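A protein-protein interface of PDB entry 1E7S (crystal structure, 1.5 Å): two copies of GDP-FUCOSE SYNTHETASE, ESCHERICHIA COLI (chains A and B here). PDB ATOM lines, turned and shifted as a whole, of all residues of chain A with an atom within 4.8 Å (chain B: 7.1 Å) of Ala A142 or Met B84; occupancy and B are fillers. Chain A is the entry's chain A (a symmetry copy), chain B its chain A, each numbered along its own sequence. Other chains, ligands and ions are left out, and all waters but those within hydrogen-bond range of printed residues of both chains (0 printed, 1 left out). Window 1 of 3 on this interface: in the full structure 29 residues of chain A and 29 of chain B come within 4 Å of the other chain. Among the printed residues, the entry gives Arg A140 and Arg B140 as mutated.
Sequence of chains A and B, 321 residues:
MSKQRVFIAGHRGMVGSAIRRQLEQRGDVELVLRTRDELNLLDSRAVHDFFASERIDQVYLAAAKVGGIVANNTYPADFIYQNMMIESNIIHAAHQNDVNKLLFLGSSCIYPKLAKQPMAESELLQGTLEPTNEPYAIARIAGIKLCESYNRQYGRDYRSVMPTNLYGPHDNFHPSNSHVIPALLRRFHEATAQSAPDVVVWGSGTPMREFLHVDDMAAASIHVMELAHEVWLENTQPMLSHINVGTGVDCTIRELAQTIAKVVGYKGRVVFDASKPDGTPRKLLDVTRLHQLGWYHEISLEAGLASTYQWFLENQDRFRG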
ATOM      1  N   MET A  84     -23.752 -25.015 -21.246  1.00  0.00           N
ATOM      2  CA  MET A  84     -22.552 -25.040 -20.408  1.00  0.00           C
ATOM      3  C   MET A  84     -22.930 -24.911 -18.933  1.00  0.00           C
ATOM      4  O   MET A  84     -22.403 -25.649 -18.090  1.00  0.00           O
ATOM      5  CB  MET A  84     -21.541 -23.967 -20.819  1.00  0.00           C
ATOM      6  CG  MET A  84     -20.846 -24.251 -22.105  1.00  0.00           C
ATOM      7  SD  MET A  84     -19.687 -22.963 -22.609  1.00  0.00           S
ATOM      8  CE  MET A  84     -18.395 -23.091 -21.360  1.00  0.00           C
ATOM      9  N   GLU A  87     -25.067 -27.917 -17.272  1.00  0.00           N
ATOM     10  CA  GLU A  87     -24.307 -29.129 -17.025  1.00  0.00           C
ATOM     11  C   GLU A  87     -23.209 -28.915 -15.982  1.00  0.00           C
ATOM     12  O   GLU A  87     -22.988 -29.786 -15.138  1.00  0.00           O
ATOM     13  CB  GLU A  87     -23.740 -29.676 -18.316  1.00  0.00           C
ATOM     14  CG  GLU A  87     -22.653 -28.909 -18.971  1.00  0.00           C
ATOM     15  CD  GLU A  87     -22.466 -29.160 -20.459  1.00  0.00           C
ATOM     16  OE1 GLU A  87     -23.132 -29.984 -21.054  1.00  0.00           O
ATOM     17  OE2 GLU A  87     -21.599 -28.461 -21.056  1.00  0.00           O
ATOM     18  N   SER A  88     -22.562 -27.748 -16.017  1.00  0.00           N
ATOM     19  CA  SER A  88     -21.495 -27.477 -15.047  1.00  0.00           C
ATOM     20  C   SER A  88     -22.064 -27.393 -13.620  1.00  0.00           C
ATOM     21  O   SER A  88     -21.532 -27.957 -12.655  1.00  0.00           O
ATOM     22  CB  SER A  88     -20.887 -26.057 -15.309  1.00  0.00           C
ATOM     23  OG  SER A  88     -20.165 -26.178 -16.516  1.00  0.00           O
ATOM     24  N   ILE A 138     -20.566 -27.960 -29.058  1.00  0.00           N
ATOM     25  CA  ILE A 138     -19.418 -27.764 -28.143  1.00  0.00           C
ATOM     26  C   ILE A 138     -19.885 -27.832 -26.690  1.00  0.00           C
ATOM     27  O   ILE A 138     -19.185 -28.446 -25.879  1.00  0.00           O
ATOM     28  CB  ILE A 138     -18.699 -26.510 -28.537  1.00  0.00           C
ATOM     29  CG1 ILE A 138     -18.011 -26.507 -29.915  1.00  0.00           C
ATOM     30  CG2 ILE A 138     -17.804 -26.044 -27.429  1.00  0.00           C
ATOM     31  CD1 ILE A 138     -16.815 -27.475 -29.852  1.00  0.00           C
ATOM     32  N   ALA A 139     -21.054 -27.227 -26.379  1.00  0.00           N
ATOM     33  CA  ALA A 139     -21.552 -27.330 -25.012  1.00  0.00           C
ATOM     34  C   ALA A 139     -21.822 -28.818 -24.654  1.00  0.00           C
ATOM     35  O   ALA A 139     -21.427 -29.248 -23.546  1.00  0.00           O
ATOM     36  CB  ALA A 139     -22.811 -26.501 -24.800  1.00  0.00           C
ATOM     37  N   ARG A 140     -22.414 -29.558 -25.583  1.00  0.00           N
ATOM     38  CA  ARG A 140     -22.679 -30.987 -25.323  1.00  0.00           C
ATOM     39  C   ARG A 140     -21.395 -31.771 -25.071  1.00  0.00           C
ATOM     40  O   ARG A 140     -21.276 -32.649 -24.188  1.00  0.00           O
ATOM     41  CB  ARG A 140     -23.557 -31.608 -26.390  1.00  0.00           C
ATOM     42  CG  ARG A 140     -25.000 -31.070 -26.448  1.00  0.00           C
ATOM     43  CD  ARG A 140     -25.707 -31.296 -25.120  1.00  0.00           C
ATOM     44  NE  ARG A 140     -27.136 -31.546 -25.286  1.00  0.00           N
ATOM     45  CZ  ARG A 140     -27.963 -31.905 -24.309  1.00  0.00           C
ATOM     46  NH1 ARG A 140     -27.554 -31.913 -23.060  1.00  0.00           N
ATOM     47  NH2 ARG A 140     -29.250 -32.246 -24.592  1.00  0.00           N
ATOM     48  N   ILE A 141     -20.402 -31.559 -25.938  1.00  0.00           N
ATOM     49  CA  ILE A 141     -19.107 -32.230 -25.798  1.00  0.00           C
ATOM     50  C   ILE A 141     -18.467 -31.861 -24.453  1.00  0.00           C
ATOM     51  O   ILE A 141     -17.940 -32.766 -23.753  1.00  0.00           O
ATOM     52  CB  ILE A 141     -18.168 -31.824 -26.950  1.00  0.00           C
ATOM     53  CG1 ILE A 141     -18.728 -32.438 -28.257  1.00  0.00           C
ATOM     54  CG2 ILE A 141     -16.759 -32.329 -26.722  1.00  0.00           C
ATOM     55  CD1 ILE A 141     -18.065 -31.945 -29.506  1.00  0.00           C
ATOM     56  N   ALA A 142     -18.567 -30.593 -24.054  1.00  0.00           N
ATOM     57  CA  ALA A 142     -18.049 -30.209 -22.745  1.00  0.00           C
ATOM     58  C   ALA A 142     -18.743 -30.999 -21.639  1.00  0.00           C
ATOM     59  O   ALA A 142     -18.094 -31.278 -20.600  1.00  0.00           O
ATOM     60  CB  ALA A 142     -18.144 -28.696 -22.552  1.00  0.00           C
ATOM     61  N   GLY A 143     -20.043 -31.296 -21.769  1.00  0.00           N
ATOM     62  CA  GLY A 143     -20.708 -32.109 -20.740  1.00  0.00           C
ATOM     63  C   GLY A 143     -20.113 -33.503 -20.643  1.00  0.00           C
ATOM     64  O   GLY A 143     -19.933 -34.014 -19.509  1.00  0.00           O
ATOM     65  N   ILE A 144     -19.869 -34.140 -21.784  1.00  0.00           N
ATOM     66  CA  ILE A 144     -19.196 -35.467 -21.744  1.00  0.00           C
ATOM     67  C   ILE A 144     -17.852 -35.344 -21.035  1.00  0.00           C
ATOM     68  O   ILE A 144     -17.497 -36.216 -20.209  1.00  0.00           O
ATOM     69  CB  ILE A 144     -18.973 -36.034 -23.164  1.00  0.00           C
ATOM     70  CG1 ILE A 144     -20.295 -36.239 -23.894  1.00  0.00           C
ATOM     71  CG2 ILE A 144     -18.182 -37.324 -23.113  1.00  0.00           C
ATOM     72  CD1 ILE A 144     -20.171 -36.555 -25.374  1.00  0.00           C
ATOM     73  N   LYS A 145     -17.077 -34.317 -21.381  1.00  0.00           N
ATOM     74  CA  LYS A 145     -15.728 -34.196 -20.844  1.00  0.00           C
ATOM     75  C   LYS A 145     -15.713 -33.804 -19.380  1.00  0.00           C
ATOM     76  O   LYS A 145     -14.797 -34.192 -18.642  1.00  0.00           O
ATOM     77  CB  LYS A 145     -14.866 -33.308 -21.764  1.00  0.00           C
ATOM     78  CG  LYS A 145     -14.777 -33.837 -23.201  1.00  0.00           C
ATOM     79  CD  LYS A 145     -14.068 -35.170 -23.242  1.00  0.00           C
ATOM     80  CE  LYS A 145     -14.178 -35.840 -24.599  1.00  0.00           C
ATOM     81  NZ  LYS A 145     -13.512 -37.202 -24.593  1.00  0.00           N
ATOM     82  N   LEU A 146     -16.773 -33.108 -18.925  1.00  0.00           N
ATOM     83  CA  LEU A 146     -16.946 -32.904 -17.467  1.00  0.00           C
ATOM     84  C   LEU A 146     -17.165 -34.255 -16.779  1.00  0.00           C
ATOM     85  O   LEU A 146     -16.510 -34.565 -15.776  1.00  0.00           O
ATOM     86  CB  LEU A 146     -18.138 -31.984 -17.178  1.00  0.00           C
ATOM     87  CG  LEU A 146     -17.822 -30.470 -17.293  1.00  0.00           C
ATOM     88  CD1 LEU A 146     -19.133 -29.729 -17.495  1.00  0.00           C
ATOM     89  CD2 LEU A 146     -17.095 -29.991 -16.043  1.00  0.00           C
ATOM     90  N   LEU B  42     -14.929 -17.670 -10.208  1.00  0.00           N
ATOM     91  CA  LEU B  42     -15.829 -18.812 -10.281  1.00  0.00           C
ATOM     92  C   LEU B  42     -17.215 -18.489  -9.720  1.00  0.00           C
ATOM     93  O   LEU B  42     -18.127 -19.265 -10.050  1.00  0.00           O
ATOM     94  CB  LEU B  42     -15.265 -19.971  -9.457  1.00  0.00           C
ATOM     95  CG  LEU B  42     -13.924 -20.514  -9.949  1.00  0.00           C
ATOM     96  CD1 LEU B  42     -13.258 -21.359  -8.856  1.00  0.00           C
ATOM     97  CD2 LEU B  42     -14.090 -21.318 -11.242  1.00  0.00           C
ATOM     98  N   ASP B  78     -10.630 -30.195 -12.379  1.00  0.00           N
ATOM     99  CA  ASP B  78     -10.318 -28.780 -12.035  1.00  0.00           C
ATOM    100  C   ASP B  78     -10.109 -27.972 -13.328  1.00  0.00           C
ATOM    101  O   ASP B  78     -10.603 -26.847 -13.456  1.00  0.00           O
ATOM    102  CB  ASP B  78      -9.033 -28.694 -11.247  1.00  0.00           C
ATOM    103  CG  ASP B  78      -8.992 -29.208  -9.855  1.00  0.00           C
ATOM    104  OD1 ASP B  78      -9.817 -29.963  -9.425  1.00  0.00           O
ATOM    105  OD2 ASP B  78      -7.920 -29.008  -9.168  1.00  0.00           O
ATOM    106  N   PHE B  79      -9.354 -28.552 -14.276  1.00  0.00           N
ATOM    107  CA  PHE B  79      -9.014 -27.786 -15.478  1.00  0.00           C
ATOM    108  C   PHE B  79     -10.201 -27.547 -16.386  1.00  0.00           C
ATOM    109  O   PHE B  79     -10.291 -26.460 -16.969  1.00  0.00           O
ATOM    110  CB  PHE B  79      -7.879 -28.508 -16.221  1.00  0.00           C
ATOM    111  CG  PHE B  79      -6.564 -28.230 -15.580  1.00  0.00           C
ATOM    112  CD1 PHE B  79      -5.864 -27.051 -15.859  1.00  0.00           C
ATOM    113  CD2 PHE B  79      -6.019 -29.112 -14.689  1.00  0.00           C
ATOM    114  CE1 PHE B  79      -4.688 -26.760 -15.201  1.00  0.00           C
ATOM    115  CE2 PHE B  79      -4.843 -28.834 -14.051  1.00  0.00           C
ATOM    116  CZ  PHE B  79      -4.116 -27.696 -14.325  1.00  0.00           C
ATOM    117  N   ILE B  80     -11.121 -28.501 -16.526  1.00  0.00           N
ATOM    118  CA  ILE B  80     -12.297 -28.253 -17.352  1.00  0.00           C
ATOM    119  C   ILE B  80     -13.303 -27.349 -16.639  1.00  0.00           C
ATOM    120  O   ILE B  80     -13.787 -26.338 -17.181  1.00  0.00           O
ATOM    121  CB  ILE B  80     -12.904 -29.502 -18.015  1.00  0.00           C
ATOM    122  CG1 ILE B  80     -14.044 -29.114 -18.931  1.00  0.00           C
ATOM    123  CG2 ILE B  80     -13.289 -30.561 -16.996  1.00  0.00           C
ATOM    124  CD1 ILE B  80     -14.462 -30.180 -19.911  1.00  0.00           C
ATOM    125  N   TYR B  81     -13.681 -27.741 -15.404  1.00  0.00           N
ATOM    126  CA  TYR B  81     -14.734 -27.020 -14.693  1.00  0.00           C
ATOM    127  C   TYR B  81     -14.340 -25.571 -14.416  1.00  0.00           C
ATOM    128  O   TYR B  81     -15.125 -24.637 -14.709  1.00  0.00           O
ATOM    129  CB  TYR B  81     -15.089 -27.697 -13.349  1.00  0.00           C
ATOM    130  CG  TYR B  81     -16.115 -26.875 -12.568  1.00  0.00           C
ATOM    131  CD1 TYR B  81     -17.470 -26.947 -12.859  1.00  0.00           C
ATOM    132  CD2 TYR B  81     -15.678 -25.995 -11.588  1.00  0.00           C
ATOM    133  CE1 TYR B  81     -18.378 -26.135 -12.190  1.00  0.00           C
ATOM    134  CE2 TYR B  81     -16.563 -25.184 -10.876  1.00  0.00           C
ATOM    135  CZ  TYR B  81     -17.929 -25.279 -11.204  1.00  0.00           C
ATOM    136  OH  TYR B  81     -18.796 -24.495 -10.482  1.00  0.00           O
ATOM    137  N   GLN B  82     -13.125 -25.326 -13.895  1.00  0.00           N
ATOM    138  CA  GLN B  82     -12.821 -23.934 -13.492  1.00  0.00           C
ATOM    139  C   GLN B  82     -12.732 -23.008 -14.675  1.00  0.00           C
ATOM    140  O   GLN B  82     -13.199 -21.867 -14.618  1.00  0.00           O
ATOM    141  CB  GLN B  82     -11.517 -23.898 -12.675  1.00  0.00           C
ATOM    142  CG  GLN B  82     -11.668 -24.592 -11.323  1.00  0.00           C
ATOM    143  CD  GLN B  82     -10.423 -24.630 -10.476  1.00  0.00           C
ATOM    144  OE1 GLN B  82      -9.600 -23.699 -10.575  1.00  0.00           O
ATOM    145  NE2 GLN B  82     -10.237 -25.663  -9.664  1.00  0.00           N
ATOM    146  N   ASN B  83     -12.126 -23.492 -15.774  1.00  0.00           N
ATOM    147  CA  ASN B  83     -12.036 -22.649 -16.981  1.00  0.00           C
ATOM    148  C   ASN B  83     -13.387 -22.434 -17.652  1.00  0.00           C
ATOM    149  O   ASN B  83     -13.671 -21.314 -18.112  1.00  0.00           O
ATOM    150  CB  ASN B  83     -10.960 -23.181 -17.901  1.00  0.00           C
ATOM    151  CG  ASN B  83      -9.584 -22.927 -17.291  1.00  0.00           C
ATOM    152  OD1 ASN B  83      -9.224 -21.792 -16.992  1.00  0.00           O
ATOM    153  ND2 ASN B  83      -8.855 -24.019 -17.108  1.00  0.00           N
ATOM    154  N   MET B  84     -14.241 -23.470 -17.686  1.00  0.00           N
ATOM    155  CA  MET B  84     -15.604 -23.251 -18.171  1.00  0.00           C
ATOM    156  C   MET B  84     -16.277 -22.130 -17.380  1.00  0.00           C
ATOM    157  O   MET B  84     -16.921 -21.253 -17.971  1.00  0.00           O
ATOM    158  CB  MET B  84     -16.439 -24.533 -18.140  1.00  0.00           C
ATOM    159  CG  MET B  84     -16.056 -25.531 -19.179  1.00  0.00           C
ATOM    160  SD  MET B  84     -17.013 -27.059 -19.110  1.00  0.00           S
ATOM    161  CE  MET B  84     -18.658 -26.510 -19.597  1.00  0.00           C
ATOM    162  N   MET B  85     -16.236 -22.200 -16.034  1.00  0.00           N
ATOM    163  CA  MET B  85     -16.993 -21.270 -15.207  1.00  0.00           C
ATOM    164  C   MET B  85     -16.415 -19.859 -15.295  1.00  0.00           C
ATOM    165  O   MET B  85     -17.175 -18.892 -15.391  1.00  0.00           O
ATOM    166  CB  MET B  85     -16.995 -21.776 -13.754  1.00  0.00           C
ATOM    167  CG  MET B  85     -17.809 -22.993 -13.474  1.00  0.00           C
ATOM    168  SD  MET B  85     -19.594 -22.824 -13.897  1.00  0.00           S
ATOM    169  CE  MET B  85     -19.880 -21.169 -13.456  1.00  0.00           C
ATOM    170  N   ILE B  86     -15.072 -19.735 -15.233  1.00  0.00           N
ATOM    171  CA  ILE B  86     -14.490 -18.372 -15.281  1.00  0.00           C
ATOM    172  C   ILE B  86     -14.905 -17.674 -16.584  1.00  0.00           C
ATOM    173  O   ILE B  86     -15.372 -16.536 -16.618  1.00  0.00           O
ATOM    174  CB  ILE B  86     -12.943 -18.473 -15.227  1.00  0.00           C
ATOM    175  CG1 ILE B  86     -12.524 -18.942 -13.818  1.00  0.00           C
ATOM    176  CG2 ILE B  86     -12.303 -17.168 -15.610  1.00  0.00           C
ATOM    177  CD1 ILE B  86     -11.044 -19.307 -13.708  1.00  0.00           C
ATOM    178  N   GLU B  87     -14.748 -18.402 -17.731  1.00  0.00           N
ATOM    179  CA  GLU B  87     -15.036 -17.752 -18.997  1.00  0.00           C
ATOM    180  C   GLU B  87     -16.531 -17.493 -19.181  1.00  0.00           C
ATOM    181  O   GLU B  87     -16.912 -16.432 -19.681  1.00  0.00           O
ATOM    182  CB  GLU B  87     -14.469 -18.552 -20.149  1.00  0.00           C
ATOM    183  CG  GLU B  87     -15.107 -19.853 -20.463  1.00  0.00           C
ATOM    184  CD  GLU B  87     -14.247 -20.846 -21.230  1.00  0.00           C
ATOM    185  OE1 GLU B  87     -13.129 -20.559 -21.611  1.00  0.00           O
ATOM    186  OE2 GLU B  87     -14.740 -21.990 -21.442  1.00  0.00           O
ATOM    187  N   SER B  88     -17.367 -18.436 -18.740  1.00  0.00           N
ATOM    188  CA  SER B  88     -18.816 -18.254 -18.888  1.00  0.00           C
ATOM    189  C   SER B  88     -19.307 -17.077 -18.028  1.00  0.00           C
ATOM    190  O   SER B  88     -20.088 -16.217 -18.457  1.00  0.00           O
ATOM    191  CB  SER B  88     -19.569 -19.501 -18.312  1.00  0.00           C
ATOM    192  OG  SER B  88     -19.308 -20.547 -19.223  1.00  0.00           O
ATOM    193  N   ASN B  89     -18.779 -17.010 -16.790  1.00  0.00           N
ATOM    194  CA  ASN B  89     -19.187 -15.926 -15.878  1.00  0.00           C
ATOM    195  C   ASN B  89     -18.813 -14.568 -16.420  1.00  0.00           C
ATOM    196  O   ASN B  89     -19.598 -13.620 -16.394  1.00  0.00           O
ATOM    197  CB  ASN B  89     -18.544 -16.132 -14.515  1.00  0.00           C
ATOM    198  CG  ASN B  89     -19.145 -17.272 -13.734  1.00  0.00           C
ATOM    199  OD1 ASN B  89     -20.263 -17.750 -14.011  1.00  0.00           O
ATOM    200  ND2 ASN B  89     -18.477 -17.676 -12.637  1.00  0.00           N
ATOM    201  N   ILE B  90     -17.535 -14.428 -16.844  1.00  0.00           N
ATOM    202  CA  ILE B  90     -17.050 -13.121 -17.322  1.00  0.00           C
ATOM    203  C   ILE B  90     -17.751 -12.678 -18.595  1.00  0.00           C
ATOM    204  O   ILE B  90     -18.156 -11.515 -18.719  1.00  0.00           O
ATOM    205  CB  ILE B  90     -15.520 -13.108 -17.504  1.00  0.00           C
ATOM    206  CG1 ILE B  90     -14.873 -13.196 -16.107  1.00  0.00           C
ATOM    207  CG2 ILE B  90     -15.063 -11.824 -18.237  1.00  0.00           C
ATOM    208  CD1 ILE B  90     -13.380 -13.461 -16.170  1.00  0.00           C
ATOM    209  N   PRO B 135      -9.249 -32.059 -21.403  1.00  0.00           N
ATOM    210  CA  PRO B 135     -10.278 -31.340 -20.628  1.00  0.00           C
ATOM    211  C   PRO B 135     -10.008 -29.841 -20.698  1.00  0.00           C
ATOM    212  O   PRO B 135     -10.929 -29.060 -20.957  1.00  0.00           O
ATOM    213  CB  PRO B 135     -10.137 -31.939 -19.232  1.00  0.00           C
ATOM    214  CG  PRO B 135      -9.591 -33.305 -19.463  1.00  0.00           C
ATOM    215  CD  PRO B 135      -8.591 -33.122 -20.603  1.00  0.00           C
ATOM    216  N   ILE B 138     -10.762 -28.446 -24.243  1.00  0.00           N
ATOM    217  CA  ILE B 138     -12.209 -28.286 -24.512  1.00  0.00           C
ATOM    218  C   ILE B 138     -12.739 -27.033 -23.816  1.00  0.00           C
ATOM    219  O   ILE B 138     -13.529 -26.312 -24.432  1.00  0.00           O
ATOM    220  CB  ILE B 138     -12.906 -29.567 -24.165  1.00  0.00           C
ATOM    221  CG1 ILE B 138     -12.559 -30.800 -25.019  1.00  0.00           C
ATOM    222  CG2 ILE B 138     -14.382 -29.343 -24.023  1.00  0.00           C
ATOM    223  CD1 ILE B 138     -13.129 -30.576 -26.432  1.00  0.00           C
ATOM    224  N   ALA B 139     -12.295 -26.777 -22.564  1.00  0.00           N
ATOM    225  CA  ALA B 139     -12.739 -25.555 -21.902  1.00  0.00           C
ATOM    226  C   ALA B 139     -12.263 -24.312 -22.704  1.00  0.00           C
ATOM    227  O   ALA B 139     -13.078 -23.383 -22.906  1.00  0.00           O
ATOM    228  CB  ALA B 139     -12.244 -25.475 -20.465  1.00  0.00           C
ATOM    229  N   ARG B 140     -11.022 -24.343 -23.174  1.00  0.00           N
ATOM    230  CA  ARG B 140     -10.509 -23.208 -23.966  1.00  0.00           C
ATOM    231  C   ARG B 140     -11.319 -22.987 -25.240  1.00  0.00           C
ATOM    232  O   ARG B 140     -11.649 -21.860 -25.670  1.00  0.00           O
ATOM    233  CB  ARG B 140      -9.019 -23.314 -24.218  1.00  0.00           C
ATOM    234  CG  ARG B 140      -8.131 -23.194 -22.966  1.00  0.00           C
ATOM    235  CD  ARG B 140      -8.359 -21.856 -22.277  1.00  0.00           C
ATOM    236  NE  ARG B 140      -7.150 -21.345 -21.639  1.00  0.00           N
ATOM    237  CZ  ARG B 140      -7.032 -20.143 -21.085  1.00  0.00           C
ATOM    238  NH1 ARG B 140      -8.085 -19.369 -20.945  1.00  0.00           N
ATOM    239  NH2 ARG B 140      -5.823 -19.710 -20.636  1.00  0.00           N
ATOM    240  N   ALA B 142     -14.364 -23.908 -25.790  1.00  0.00           N
ATOM    241  CA  ALA B 142     -15.665 -23.363 -25.413  1.00  0.00           C
ATOM    242  C   ALA B 142     -15.576 -21.852 -25.213  1.00  0.00           C
ATOM    243  O   ALA B 142     -16.582 -21.149 -25.482  1.00  0.00           O
ATOM    244  CB  ALA B 142     -16.223 -24.098 -24.196  1.00  0.00           C
ATOM    245  N   GLY B 143     -14.465 -21.330 -24.676  1.00  0.00           N
ATOM    246  CA  GLY B 143     -14.343 -19.872 -24.533  1.00  0.00           C
ATOM    247  C   GLY B 143     -14.360 -19.166 -25.878  1.00  0.00           C
ATOM    248  O   GLY B 143     -15.009 -18.096 -25.999  1.00  0.00           O
ATOM    249  N   LEU B 146     -17.936 -19.280 -27.088  1.00  0.00           N
ATOM    250  CA  LEU B 146     -18.770 -18.286 -26.371  1.00  0.00           C
ATOM    251  C   LEU B 146     -18.579 -16.903 -27.001  1.00  0.00           C
ATOM    252  O   LEU B 146     -19.557 -16.209 -27.308  1.00  0.00           O
ATOM    253  CB  LEU B 146     -18.403 -18.227 -24.885  1.00  0.00           C
ATOM    254  CG  LEU B 146     -19.069 -19.325 -24.015  1.00  0.00           C
ATOM    255  CD1 LEU B 146     -18.255 -19.475 -22.741  1.00  0.00           C
ATOM    256  CD2 LEU B 146     -20.514 -18.950 -23.716  1.00  0.00           C
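Met A84 touches its own counterpart, Met B84. Met A84 touches Glu B87, and with the chains exchanged Glu A87 touches Met B84. Met A84 touches Ala B142, and with the chains exchanged Ala A142 touches Met B84. Ile A138 touches Ala B142, and with the chains exchanged Ala A142 touches Ile B138. Positions printed for both chains: 84, 87, 88, 138, 139, 140, 142, 143 and 146. Of the 16 pairs that touch across the chains among the printed residues, 11 have their exchanged pair printed and touching as well.
Among the printed residues, merely in contact across the chains: Met A84 with Ser B88 (3.4 Å), Ser A88 with Met B84 (3.4 Å), Lys A145 with Ile B80 (3.7 Å), Ser A88 with Tyr B81 (3.7 Å), Met A84 with Ala B142 (3.7 Å), Ala A142 with Met B84 (3.7 Å), Ser A88 with Met B85 (3.8 Å), Leu A146 with Met B84 (3.8 Å), Met A84 with Leu B146 (3.8 Å), Met A84 with Glu B87 (3.8 Å), Glu A87 with Met B84 (3.8 Å), Met A84 with Met B84 (3.9 Å), Ala A142 with Ile B80 (3.9 Å), Leu A146 with Ile B80 (3.9 Å), Ile A138 with Ala B142 (3.98 Å) and Ala A142 with Ile B138 (3.98 Å).
Of the 12 printed residues of chain A, 7 touch a printed residue of chain B. Printed residues of chain A that touch a printed residue of chain B: Met A84, Glu A87, Ser A88, Ile A138, Ala A142, Lys A145 and Leu A146. Among the printed residues, no Asp or Glu carboxylate lies within 4 Å of a Lys or Arg side-chain nitrogen of the other chain.
Ala A142 touches just these residues of chain B: Ile B80 (3.9 Å), Met B84 (3.7 Å) and Ile B138 (3.98 Å). Of the printed residues of chain A, Ile B80 touches Ala A142 (3.9 Å), Lys A145 (3.7 Å) and Leu A146 (3.9 Å). Printed residues of chain A within 4 Å of Met B85: Ser A88. Arg B140 touches none of the printed residues of chain A. The nearest printed residue of chain A that does not touch Met B84 is Gly A143 (5.4 Å).
The side-chain carboxylate of Glu B87 lies close to the backbone carbonyl oxygen of Ala B139, 2.6 Å away. The backbone carbonyl oxygen (O) of Met A84 is in hydrogen-bond range of the side-chain hydroxyl (OG) of Ser A88 (2.8 Å). The side-chain carboxylate (OE2) of Glu A87 is in hydrogen-bond range of the backbone NH (N) of Gly A143 (3.3 Å). O of Met B84 lies within hydrogen-bond range of OG of Ser B88, at 2.8 Å. The backbone carbonyl oxygen (O) of Met B85 sits close to the side-chain amide nitrogen (ND2) of Asn B89 (3.3 Å). The side-chain carboxylate (OE2) of Glu B87 is in hydrogen-bond range of the backbone NH (N) of Gly B143 (3.3 Å).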
